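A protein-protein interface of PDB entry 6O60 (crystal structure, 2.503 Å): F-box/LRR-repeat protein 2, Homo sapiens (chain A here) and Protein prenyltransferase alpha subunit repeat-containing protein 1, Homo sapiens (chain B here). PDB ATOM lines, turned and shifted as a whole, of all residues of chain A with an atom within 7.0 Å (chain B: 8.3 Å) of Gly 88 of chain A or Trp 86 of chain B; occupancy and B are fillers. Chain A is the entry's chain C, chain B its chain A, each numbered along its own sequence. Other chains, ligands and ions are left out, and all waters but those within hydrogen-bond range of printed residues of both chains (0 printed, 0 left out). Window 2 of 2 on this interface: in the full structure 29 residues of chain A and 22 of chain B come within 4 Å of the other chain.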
ATOM      1  N   LEU A  58       9.000   6.046   7.286  1.00  0.00           N
ATOM      2  CA  LEU A  58       9.207   5.032   6.257  1.00  0.00           C
ATOM      3  C   LEU A  58      10.043   3.856   6.769  1.00  0.00           C
ATOM      4  O   LEU A  58      11.157   4.047   7.262  1.00  0.00           O
ATOM      5  CB  LEU A  58       9.883   5.670   5.048  1.00  0.00           C
ATOM      6  CG  LEU A  58       8.959   6.490   4.152  1.00  0.00           C
ATOM      7  CD1 LEU A  58       9.571   6.632   2.773  1.00  0.00           C
ATOM      8  CD2 LEU A  58       7.574   5.855   4.056  1.00  0.00           C
ATOM      9  N   GLN A  62      14.893   0.022  -0.444  1.00  0.00           N
ATOM     10  CA  GLN A  62      15.684   1.142  -0.954  1.00  0.00           C
ATOM     11  C   GLN A  62      15.255   1.542  -2.362  1.00  0.00           C
ATOM     12  O   GLN A  62      14.829   2.680  -2.591  1.00  0.00           O
ATOM     13  CB  GLN A  62      17.170   0.792  -0.924  1.00  0.00           C
ATOM     14  CG  GLN A  62      17.626   0.143   0.369  1.00  0.00           C
ATOM     15  CD  GLN A  62      19.060  -0.353   0.285  1.00  0.00           C
ATOM     16  OE1 GLN A  62      19.856   0.155  -0.508  1.00  0.00           O
ATOM     17  NE2 GLN A  62      19.396  -1.348   1.102  1.00  0.00           N
ATOM     18  N   SER A  85      10.016  11.084   8.816  1.00  0.00           N
ATOM     19  CA  SER A  85      11.229  10.396   9.220  1.00  0.00           C
ATOM     20  C   SER A  85      11.717   9.560   8.047  1.00  0.00           C
ATOM     21  O   SER A  85      10.938   8.820   7.437  1.00  0.00           O
ATOM     22  CB  SER A  85      10.987   9.525  10.451  1.00  0.00           C
ATOM     23  OG  SER A  85      12.208   8.941  10.900  1.00  0.00           O
ATOM     24  N   LEU A  86      12.990   9.716   7.706  1.00  0.00           N
ATOM     25  CA  LEU A  86      13.637   8.920   6.673  1.00  0.00           C
ATOM     26  C   LEU A  86      14.896   8.263   7.212  1.00  0.00           C
ATOM     27  O   LEU A  86      15.817   7.972   6.453  1.00  0.00           O
ATOM     28  CB  LEU A  86      13.980   9.770   5.455  1.00  0.00           C
ATOM     29  CG  LEU A  86      12.799  10.338   4.687  1.00  0.00           C
ATOM     30  CD1 LEU A  86      13.322  10.910   3.397  1.00  0.00           C
ATOM     31  CD2 LEU A  86      11.787   9.208   4.452  1.00  0.00           C
ATOM     32  N   ARG A  87      14.945   8.041   8.524  1.00  0.00           N
ATOM     33  CA  ARG A  87      16.132   7.495   9.166  1.00  0.00           C
ATOM     34  C   ARG A  87      16.541   6.163   8.548  1.00  0.00           C
ATOM     35  O   ARG A  87      15.770   5.203   8.527  1.00  0.00           O
ATOM     36  CB  ARG A  87      15.896   7.333  10.674  1.00  0.00           C
ATOM     37  CG  ARG A  87      17.011   6.593  11.373  1.00  0.00           C
ATOM     38  CD  ARG A  87      16.580   6.102  12.731  1.00  0.00           C
ATOM     39  NE  ARG A  87      15.657   7.038  13.352  1.00  0.00           N
ATOM     40  CZ  ARG A  87      14.934   6.765  14.433  1.00  0.00           C
ATOM     41  NH1 ARG A  87      14.118   7.693  14.940  1.00  0.00           N
ATOM     42  NH2 ARG A  87      15.018   5.559  14.992  1.00  0.00           N
ATOM     43  N   GLY A  88      17.765   6.121   8.044  1.00  0.00           N
ATOM     44  CA  GLY A  88      18.331   4.944   7.447  1.00  0.00           C
ATOM     45  C   GLY A  88      17.856   4.652   6.046  1.00  0.00           C
ATOM     46  O   GLY A  88      18.230   3.617   5.491  1.00  0.00           O
ATOM     47  N   CYS A  89      17.022   5.506   5.458  1.00  0.00           N
ATOM     48  CA  CYS A  89      16.620   5.341   4.062  1.00  0.00           C
ATOM     49  C   CYS A  89      17.751   5.831   3.157  1.00  0.00           C
ATOM     50  O   CYS A  89      17.705   6.923   2.584  1.00  0.00           O
ATOM     51  CB  CYS A  89      15.321   6.090   3.784  1.00  0.00           C
ATOM     52  SG  CYS A  89      13.972   5.648   4.881  1.00  0.00           S
ATOM     53  N   ILE A  90      18.793   4.998   3.026  1.00  0.00           N
ATOM     54  CA  ILE A  90      19.901   5.320   2.119  1.00  0.00           C
ATOM     55  C   ILE A  90      19.420   5.399   0.666  1.00  0.00           C
ATOM     56  O   ILE A  90      20.086   6.007  -0.181  1.00  0.00           O
ATOM     57  CB  ILE A  90      21.069   4.312   2.274  1.00  0.00           C
ATOM     58  CG1 ILE A  90      21.893   4.577   3.538  1.00  0.00           C
ATOM     59  CG2 ILE A  90      22.064   4.409   1.124  1.00  0.00           C
ATOM     60  CD1 ILE A  90      21.329   4.055   4.802  1.00  0.00           C
ATOM     61  N   GLY A  91      18.244   4.854   0.357  1.00  0.00           N
ATOM     62  CA  GLY A  91      17.709   5.004  -0.989  1.00  0.00           C
ATOM     63  C   GLY A  91      17.602   6.453  -1.443  1.00  0.00           C
ATOM     64  O   GLY A  91      17.904   6.772  -2.596  1.00  0.00           O
ATOM     65  N   VAL A  92      17.191   7.352  -0.541  1.00  0.00           N
ATOM     66  CA  VAL A  92      16.815   8.707  -0.945  1.00  0.00           C
ATOM     67  C   VAL A  92      18.055   9.550  -1.233  1.00  0.00           C
ATOM     68  O   VAL A  92      19.053   9.517  -0.495  1.00  0.00           O
ATOM     69  CB  VAL A  92      15.921   9.369   0.125  1.00  0.00           C
ATOM     70  CG1 VAL A  92      14.659   8.545   0.366  1.00  0.00           C
ATOM     71  CG2 VAL A  92      16.677   9.605   1.435  1.00  0.00           C
ATOM     72  N   ASN A 111      13.629  14.145   9.491  1.00  0.00           N
ATOM     73  CA  ASN A 111      14.692  13.303  10.019  1.00  0.00           C
ATOM     74  C   ASN A 111      15.401  12.599   8.865  1.00  0.00           C
ATOM     75  O   ASN A 111      14.861  11.654   8.278  1.00  0.00           O
ATOM     76  CB  ASN A 111      14.130  12.296  11.013  1.00  0.00           C
ATOM     77  CG  ASN A 111      15.219  11.621  11.835  1.00  0.00           C
ATOM     78  OD1 ASN A 111      16.345  11.410  11.378  1.00  0.00           O
ATOM     79  ND2 ASN A 111      14.875  11.274  13.053  1.00  0.00           N
ATOM     80  N   LEU A 112      16.623  13.040   8.561  1.00  0.00           N
ATOM     81  CA  LEU A 112      17.411  12.447   7.487  1.00  0.00           C
ATOM     82  C   LEU A 112      18.590  11.632   8.018  1.00  0.00           C
ATOM     83  O   LEU A 112      19.582  11.444   7.307  1.00  0.00           O
ATOM     84  CB  LEU A 112      17.895  13.532   6.530  1.00  0.00           C
ATOM     85  CG  LEU A 112      16.785  14.405   5.937  1.00  0.00           C
ATOM     86  CD1 LEU A 112      17.390  15.558   5.157  1.00  0.00           C
ATOM     87  CD2 LEU A 112      15.833  13.578   5.046  1.00  0.00           C
ATOM     88  N   ASN A 113      18.490  11.147   9.250  1.00  0.00           N
ATOM     89  CA  ASN A 113      19.555  10.391   9.903  1.00  0.00           C
ATOM     90  C   ASN A 113      20.052   9.252   9.017  1.00  0.00           C
ATOM     91  O   ASN A 113      19.279   8.381   8.615  1.00  0.00           O
ATOM     92  CB  ASN A 113      19.010   9.852  11.224  1.00  0.00           C
ATOM     93  CG  ASN A 113      20.081   9.312  12.146  1.00  0.00           C
ATOM     94  OD1 ASN A 113      21.113   8.794  11.716  1.00  0.00           O
ATOM     95  ND2 ASN A 113      19.817   9.408  13.432  1.00  0.00           N
ATOM     96  N   GLY A 114      21.342   9.274   8.694  1.00  0.00           N
ATOM     97  CA  GLY A 114      21.940   8.229   7.898  1.00  0.00           C
ATOM     98  C   GLY A 114      21.690   8.295   6.407  1.00  0.00           C
ATOM     99  O   GLY A 114      22.183   7.425   5.675  1.00  0.00           O
ATOM    100  N   CYS A 115      20.943   9.279   5.916  1.00  0.00           N
ATOM    101  CA  CYS A 115      20.741   9.376   4.472  1.00  0.00           C
ATOM    102  C   CYS A 115      22.007   9.912   3.814  1.00  0.00           C
ATOM    103  O   CYS A 115      22.205  11.125   3.688  1.00  0.00           O
ATOM    104  CB  CYS A 115      19.522  10.235   4.167  1.00  0.00           C
ATOM    105  SG  CYS A 115      18.048   9.566   4.968  1.00  0.00           S
ATOM    106  N   THR A 139      22.054  13.803  11.246  1.00  0.00           N
ATOM    107  CA  THR A 139      22.986  12.791  11.727  1.00  0.00           C
ATOM    108  C   THR A 139      23.529  11.952  10.578  1.00  0.00           C
ATOM    109  O   THR A 139      22.765  11.371   9.792  1.00  0.00           O
ATOM    110  CB  THR A 139      22.289  11.886  12.757  1.00  0.00           C
ATOM    111  OG1 THR A 139      21.718  12.684  13.802  1.00  0.00           O
ATOM    112  CG2 THR A 139      23.269  10.903  13.366  1.00  0.00           C
ATOM    113  N   SER A 140      24.851  11.945  10.455  1.00  0.00           N
ATOM    114  CA  SER A 140      25.591  11.087   9.538  1.00  0.00           C
ATOM    115  C   SER A 140      25.340  11.415   8.080  1.00  0.00           C
ATOM    116  O   SER A 140      25.620  10.600   7.208  1.00  0.00           O
ATOM    117  CB  SER A 140      25.298   9.609   9.805  1.00  0.00           C
ATOM    118  OG  SER A 140      25.831   9.256  11.068  1.00  0.00           O
ATOM    119  N   TRP A 166      28.121  13.708  13.678  1.00  0.00           N
ATOM    120  CA  TRP A 166      29.026  13.028  12.745  1.00  0.00           C
ATOM    121  C   TRP A 166      29.002  13.645  11.350  1.00  0.00           C
ATOM    122  O   TRP A 166      29.317  12.974  10.362  1.00  0.00           O
ATOM    123  CB  TRP A 166      28.738  11.522  12.679  1.00  0.00           C
ATOM    124  CG  TRP A 166      28.934  10.901  14.017  1.00  0.00           C
ATOM    125  CD1 TRP A 166      30.114  10.816  14.717  1.00  0.00           C
ATOM    126  CD2 TRP A 166      27.926  10.333  14.860  1.00  0.00           C
ATOM    127  NE1 TRP A 166      29.898  10.215  15.936  1.00  0.00           N
ATOM    128  CE2 TRP A 166      28.568   9.904  16.050  1.00  0.00           C
ATOM    129  CE3 TRP A 166      26.550  10.119  14.719  1.00  0.00           C
ATOM    130  CZ2 TRP A 166      27.878   9.266  17.092  1.00  0.00           C
ATOM    131  CZ3 TRP A 166      25.859   9.478  15.760  1.00  0.00           C
ATOM    132  CH2 TRP A 166      26.527   9.066  16.929  1.00  0.00           C
ATOM    133  N   LYS B  76      21.819  -7.800  16.865  1.00  0.00           N
ATOM    134  CA  LYS B  76      21.816  -6.344  16.793  1.00  0.00           C
ATOM    135  C   LYS B  76      22.168  -5.899  15.383  1.00  0.00           C
ATOM    136  O   LYS B  76      21.483  -5.057  14.799  1.00  0.00           O
ATOM    137  CB  LYS B  76      22.793  -5.754  17.808  1.00  0.00           C
ATOM    138  CG  LYS B  76      22.200  -5.490  19.181  1.00  0.00           C
ATOM    139  CD  LYS B  76      21.133  -4.423  19.112  1.00  0.00           C
ATOM    140  CE  LYS B  76      20.520  -4.120  20.473  1.00  0.00           C
ATOM    141  NZ  LYS B  76      21.385  -3.235  21.308  1.00  0.00           N
ATOM    142  N   LEU B  79      19.213  -6.676  13.038  1.00  0.00           N
ATOM    143  CA  LEU B  79      18.049  -5.816  13.233  1.00  0.00           C
ATOM    144  C   LEU B  79      18.276  -4.451  12.601  1.00  0.00           C
ATOM    145  O   LEU B  79      17.351  -3.853  12.036  1.00  0.00           O
ATOM    146  CB  LEU B  79      17.732  -5.703  14.723  1.00  0.00           C
ATOM    147  CG  LEU B  79      17.147  -6.986  15.338  1.00  0.00           C
ATOM    148  CD1 LEU B  79      17.182  -6.933  16.840  1.00  0.00           C
ATOM    149  CD2 LEU B  79      15.737  -7.182  14.860  1.00  0.00           C
ATOM    150  N   TYR B  80      19.515  -3.958  12.664  1.00  0.00           N
ATOM    151  CA  TYR B  80      19.919  -2.763  11.926  1.00  0.00           C
ATOM    152  C   TYR B  80      19.759  -2.961  10.427  1.00  0.00           C
ATOM    153  O   TYR B  80      19.059  -2.197   9.752  1.00  0.00           O
ATOM    154  CB  TYR B  80      21.373  -2.431  12.260  1.00  0.00           C
ATOM    155  CG  TYR B  80      21.990  -1.366  11.392  1.00  0.00           C
ATOM    156  CD1 TYR B  80      21.670  -0.025  11.576  1.00  0.00           C
ATOM    157  CD2 TYR B  80      22.915  -1.695  10.409  1.00  0.00           C
ATOM    158  CE1 TYR B  80      22.242   0.960  10.798  1.00  0.00           C
ATOM    159  CE2 TYR B  80      23.497  -0.719   9.628  1.00  0.00           C
ATOM    160  CZ  TYR B  80      23.153   0.612   9.823  1.00  0.00           C
ATOM    161  OH  TYR B  80      23.722   1.601   9.040  1.00  0.00           O
ATOM    162  N   ARG B  81      20.408  -3.999   9.891  1.00  0.00           N
ATOM    163  CA  ARG B  81      20.377  -4.250   8.459  1.00  0.00           C
ATOM    164  C   ARG B  81      18.961  -4.457   7.968  1.00  0.00           C
ATOM    165  O   ARG B  81      18.641  -4.134   6.822  1.00  0.00           O
ATOM    166  CB  ARG B  81      21.227  -5.473   8.133  1.00  0.00           C
ATOM    167  CG  ARG B  81      22.552  -5.112   7.529  1.00  0.00           C
ATOM    168  CD  ARG B  81      22.406  -4.768   6.076  1.00  0.00           C
ATOM    169  NE  ARG B  81      23.711  -4.552   5.479  1.00  0.00           N
ATOM    170  CZ  ARG B  81      24.255  -3.368   5.259  1.00  0.00           C
ATOM    171  NH1 ARG B  81      25.460  -3.293   4.715  1.00  0.00           N
ATOM    172  NH2 ARG B  81      23.587  -2.260   5.548  1.00  0.00           N
ATOM    173  N   ARG B  83      16.319  -3.050   9.287  1.00  0.00           N
ATOM    174  CA  ARG B  83      15.593  -1.799   9.509  1.00  0.00           C
ATOM    175  C   ARG B  83      14.564  -1.904  10.640  1.00  0.00           C
ATOM    176  O   ARG B  83      13.543  -1.209  10.615  1.00  0.00           O
ATOM    177  CB  ARG B  83      14.923  -1.308   8.216  1.00  0.00           C
ATOM    178  CG  ARG B  83      15.885  -0.734   7.167  1.00  0.00           C
ATOM    179  CD  ARG B  83      16.022   0.783   7.305  1.00  0.00           C
ATOM    180  NE  ARG B  83      14.871   1.514   6.759  1.00  0.00           N
ATOM    181  CZ  ARG B  83      14.685   1.780   5.466  1.00  0.00           C
ATOM    182  NH1 ARG B  83      15.574   1.373   4.561  1.00  0.00           N
ATOM    183  NH2 ARG B  83      13.602   2.445   5.074  1.00  0.00           N
ATOM    184  N   LYS B  84      14.826  -2.735  11.659  1.00  0.00           N
ATOM    185  CA  LYS B  84      13.943  -2.839  12.826  1.00  0.00           C
ATOM    186  C   LYS B  84      14.524  -2.246  14.111  1.00  0.00           C
ATOM    187  O   LYS B  84      13.772  -2.042  15.078  1.00  0.00           O
ATOM    188  CB  LYS B  84      13.563  -4.307  13.095  1.00  0.00           C
ATOM    189  CG  LYS B  84      13.063  -5.052  11.865  1.00  0.00           C
ATOM    190  CD  LYS B  84      12.129  -6.222  12.200  1.00  0.00           C
ATOM    191  CE  LYS B  84      10.789  -5.754  12.769  1.00  0.00           C
ATOM    192  NZ  LYS B  84       9.650  -6.702  12.560  1.00  0.00           N
ATOM    193  N   GLN B  85      15.827  -1.976  14.167  1.00  0.00           N
ATOM    194  CA  GLN B  85      16.407  -1.315  15.330  1.00  0.00           C
ATOM    195  C   GLN B  85      17.600  -0.506  14.861  1.00  0.00           C
ATOM    196  O   GLN B  85      18.459  -1.033  14.158  1.00  0.00           O
ATOM    197  CB  GLN B  85      16.832  -2.313  16.403  1.00  0.00           C
ATOM    198  CG  GLN B  85      15.927  -2.357  17.617  1.00  0.00           C
ATOM    199  CD  GLN B  85      16.274  -3.507  18.547  1.00  0.00           C
ATOM    200  OE1 GLN B  85      17.416  -3.633  19.011  1.00  0.00           O
ATOM    201  NE2 GLN B  85      15.297  -4.373  18.798  1.00  0.00           N
ATOM    202  N   TRP B  86      17.647   0.760  15.239  1.00  0.00           N
ATOM    203  CA  TRP B  86      18.675   1.656  14.745  1.00  0.00           C
ATOM    204  C   TRP B  86      19.934   1.547  15.589  1.00  0.00           C
ATOM    205  O   TRP B  86      19.871   1.371  16.811  1.00  0.00           O
ATOM    206  CB  TRP B  86      18.178   3.102  14.752  1.00  0.00           C
ATOM    207  CG  TRP B  86      19.117   4.069  14.075  1.00  0.00           C
ATOM    208  CD1 TRP B  86      19.765   5.110  14.655  1.00  0.00           C
ATOM    209  CD2 TRP B  86      19.508   4.072  12.690  1.00  0.00           C
ATOM    210  NE1 TRP B  86      20.532   5.770  13.725  1.00  0.00           N
ATOM    211  CE2 TRP B  86      20.390   5.155  12.510  1.00  0.00           C
ATOM    212  CE3 TRP B  86      19.199   3.263  11.590  1.00  0.00           C
ATOM    213  CZ2 TRP B  86      20.971   5.449  11.274  1.00  0.00           C
ATOM    214  CZ3 TRP B  86      19.784   3.548  10.368  1.00  0.00           C
ATOM    215  CH2 TRP B  86      20.654   4.637  10.218  1.00  0.00           C
ATOM    216  N   LEU B  87      21.084   1.652  14.933  1.00  0.00           N
ATOM    217  CA  LEU B  87      22.338   1.879  15.625  1.00  0.00           C
ATOM    218  C   LEU B  87      23.000   3.124  15.043  1.00  0.00           C
ATOM    219  O   LEU B  87      22.973   3.357  13.827  1.00  0.00           O
ATOM    220  CB  LEU B  87      23.256   0.647  15.543  1.00  0.00           C
ATOM    221  CG  LEU B  87      22.628  -0.646  16.098  1.00  0.00           C
ATOM    222  CD1 LEU B  87      23.120  -1.845  15.342  1.00  0.00           C
ATOM    223  CD2 LEU B  87      22.896  -0.809  17.577  1.00  0.00           C
ATOM    224  N   ASN B  88      23.548   3.948  15.927  1.00  0.00           N
ATOM    225  CA  ASN B  88      24.279   5.118  15.495  1.00  0.00           C
ATOM    226  C   ASN B  88      25.693   4.717  15.078  1.00  0.00           C
ATOM    227  O   ASN B  88      26.081   3.550  15.124  1.00  0.00           O
ATOM    228  CB  ASN B  88      24.273   6.190  16.590  1.00  0.00           C
ATOM    229  CG  ASN B  88      25.005   5.765  17.861  1.00  0.00           C
ATOM    230  OD1 ASN B  88      26.181   5.368  17.841  1.00  0.00           O
ATOM    231  ND2 ASN B  88      24.317   5.880  18.983  1.00  0.00           N
ATOM    232  N   ARG B  89      26.474   5.721  14.689  1.00  0.00           N
ATOM    233  CA  ARG B  89      27.776   5.494  14.074  1.00  0.00           C
ATOM    234  C   ARG B  89      28.721   4.771  15.033  1.00  0.00           C
ATOM    235  O   ARG B  89      29.376   3.783  14.664  1.00  0.00           O
ATOM    236  CB  ARG B  89      28.326   6.855  13.637  1.00  0.00           C
ATOM    237  CG  ARG B  89      29.686   6.869  13.058  1.00  0.00           C
ATOM    238  CD  ARG B  89      30.626   7.399  14.074  1.00  0.00           C
ATOM    239  NE  ARG B  89      31.936   7.645  13.508  1.00  0.00           N
ATOM    240  CZ  ARG B  89      33.048   7.514  14.208  1.00  0.00           C
ATOM    241  NH1 ARG B  89      32.976   7.136  15.480  1.00  0.00           N
ATOM    242  NH2 ARG B  89      34.221   7.747  13.638  1.00  0.00           N
ATOM    243  N   GLU B  91      27.956   2.910  17.609  1.00  0.00           N
ATOM    244  CA  GLU B  91      27.510   1.560  17.917  1.00  0.00           C
ATOM    245  C   GLU B  91      27.755   0.628  16.746  1.00  0.00           C
ATOM    246  O   GLU B  91      28.222  -0.499  16.931  1.00  0.00           O
ATOM    247  CB  GLU B  91      26.036   1.576  18.293  1.00  0.00           C
ATOM    248  CG  GLU B  91      25.768   2.313  19.577  1.00  0.00           C
ATOM    249  CD  GLU B  91      24.293   2.590  19.785  1.00  0.00           C
ATOM    250  OE1 GLU B  91      23.871   2.608  20.961  1.00  0.00           O
ATOM    251  OE2 GLU B  91      23.563   2.804  18.782  1.00  0.00           O
ATOM    252  N   LEU B  92      27.451   1.088  15.534  1.00  0.00           N
ATOM    253  CA  LEU B  92      27.794   0.333  14.343  1.00  0.00           C
ATOM    254  C   LEU B  92      29.245  -0.113  14.394  1.00  0.00           C
ATOM    255  O   LEU B  92      29.545  -1.310  14.317  1.00  0.00           O
ATOM    256  CB  LEU B  92      27.530   1.184  13.106  1.00  0.00           C
ATOM    257  CG  LEU B  92      26.278   0.787  12.334  1.00  0.00           C
ATOM    258  CD1 LEU B  92      26.339   1.393  10.946  1.00  0.00           C
ATOM    259  CD2 LEU B  92      26.100  -0.759  12.278  1.00  0.00           C
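The side-chain sulfur (SG) of Cys 89 of chain A lies within hydrogen-bond range of the guanidinium group (NH2) of Arg 83 of chain B.
Among the printed residues, pairs that only touch across the chains: Asn 113 of chain A with Trp 86 of chain B (3.4 Å), Trp 166 of chain A with Arg 89 of chain B (3.5 Å), Arg 87 of chain A with Trp 86 of chain B (3.5 Å), Gly 88 of chain A with Trp 86 of chain B (3.5 Å), Gly 88 of chain A with Arg 83 of chain B (3.6 Å), Leu 58 of chain A with Arg 83 of chain B (3.7 Å) and Trp 166 of chain A with Asn 88 of chain B (3.7 Å).
Trp 86 of chain B touches three residues of chain A. Of chain B, only Arg 83 comes within 4 Å of Cys 89 of chain A. Of the printed residues of chain A, Arg 83 of chain B touches Leu 58 (3.7 Å), Gly 88 (3.6 Å) and Cys 89 (3.2 Å). Printed residues of chain A within 4 Å of Arg 89 of chain B: Trp 166. Printed residues of chain B within 4 Å of Leu 58 of chain A: Arg 83. The nearest printed residue of chain B that does not touch Trp 166 of chain A is Glu 91 of chain B (6.4 Å).
O of Cys 89 of chain A sits at hydrogen-bond distance from SG of Cys 115 of chain A (3.6 Å). The backbone NH (N) of Asn 113 of chain A sits at hydrogen-bond distance from the side-chain amide oxygen (OD1) of Asn 111 of chain A. The side-chain amide oxygen of Asn 88 of chain B sits at hydrogen-bond distance from the backbone NH of Glu 91 of chain B, at 3.0 Å. N of Leu 58 of chain A lies within hydrogen-bond range of O of Ser 85 of chain A, at 3.4 Å. The side-chain sulfur (SG) of Cys 89 of chain A sits close to the backbone carbonyl oxygen (O) of Leu 86 of chain A (3.4 Å). The backbone NH (N) of Gly 88 of chain A is in hydrogen-bond range of the backbone carbonyl oxygen (O) of Asn 113 of chain A, at 2.8 Å.
Of the 18 printed residues of chain A, 6 touch a printed residue of chain B. Hydrophobic or aromatic side chains of chain A that line the printed part of chain B: Trp 166. Among the printed residues, no Asp or Glu carboxylate lies within 4 Å of a Lys or Arg side-chain nitrogen of the other chain.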
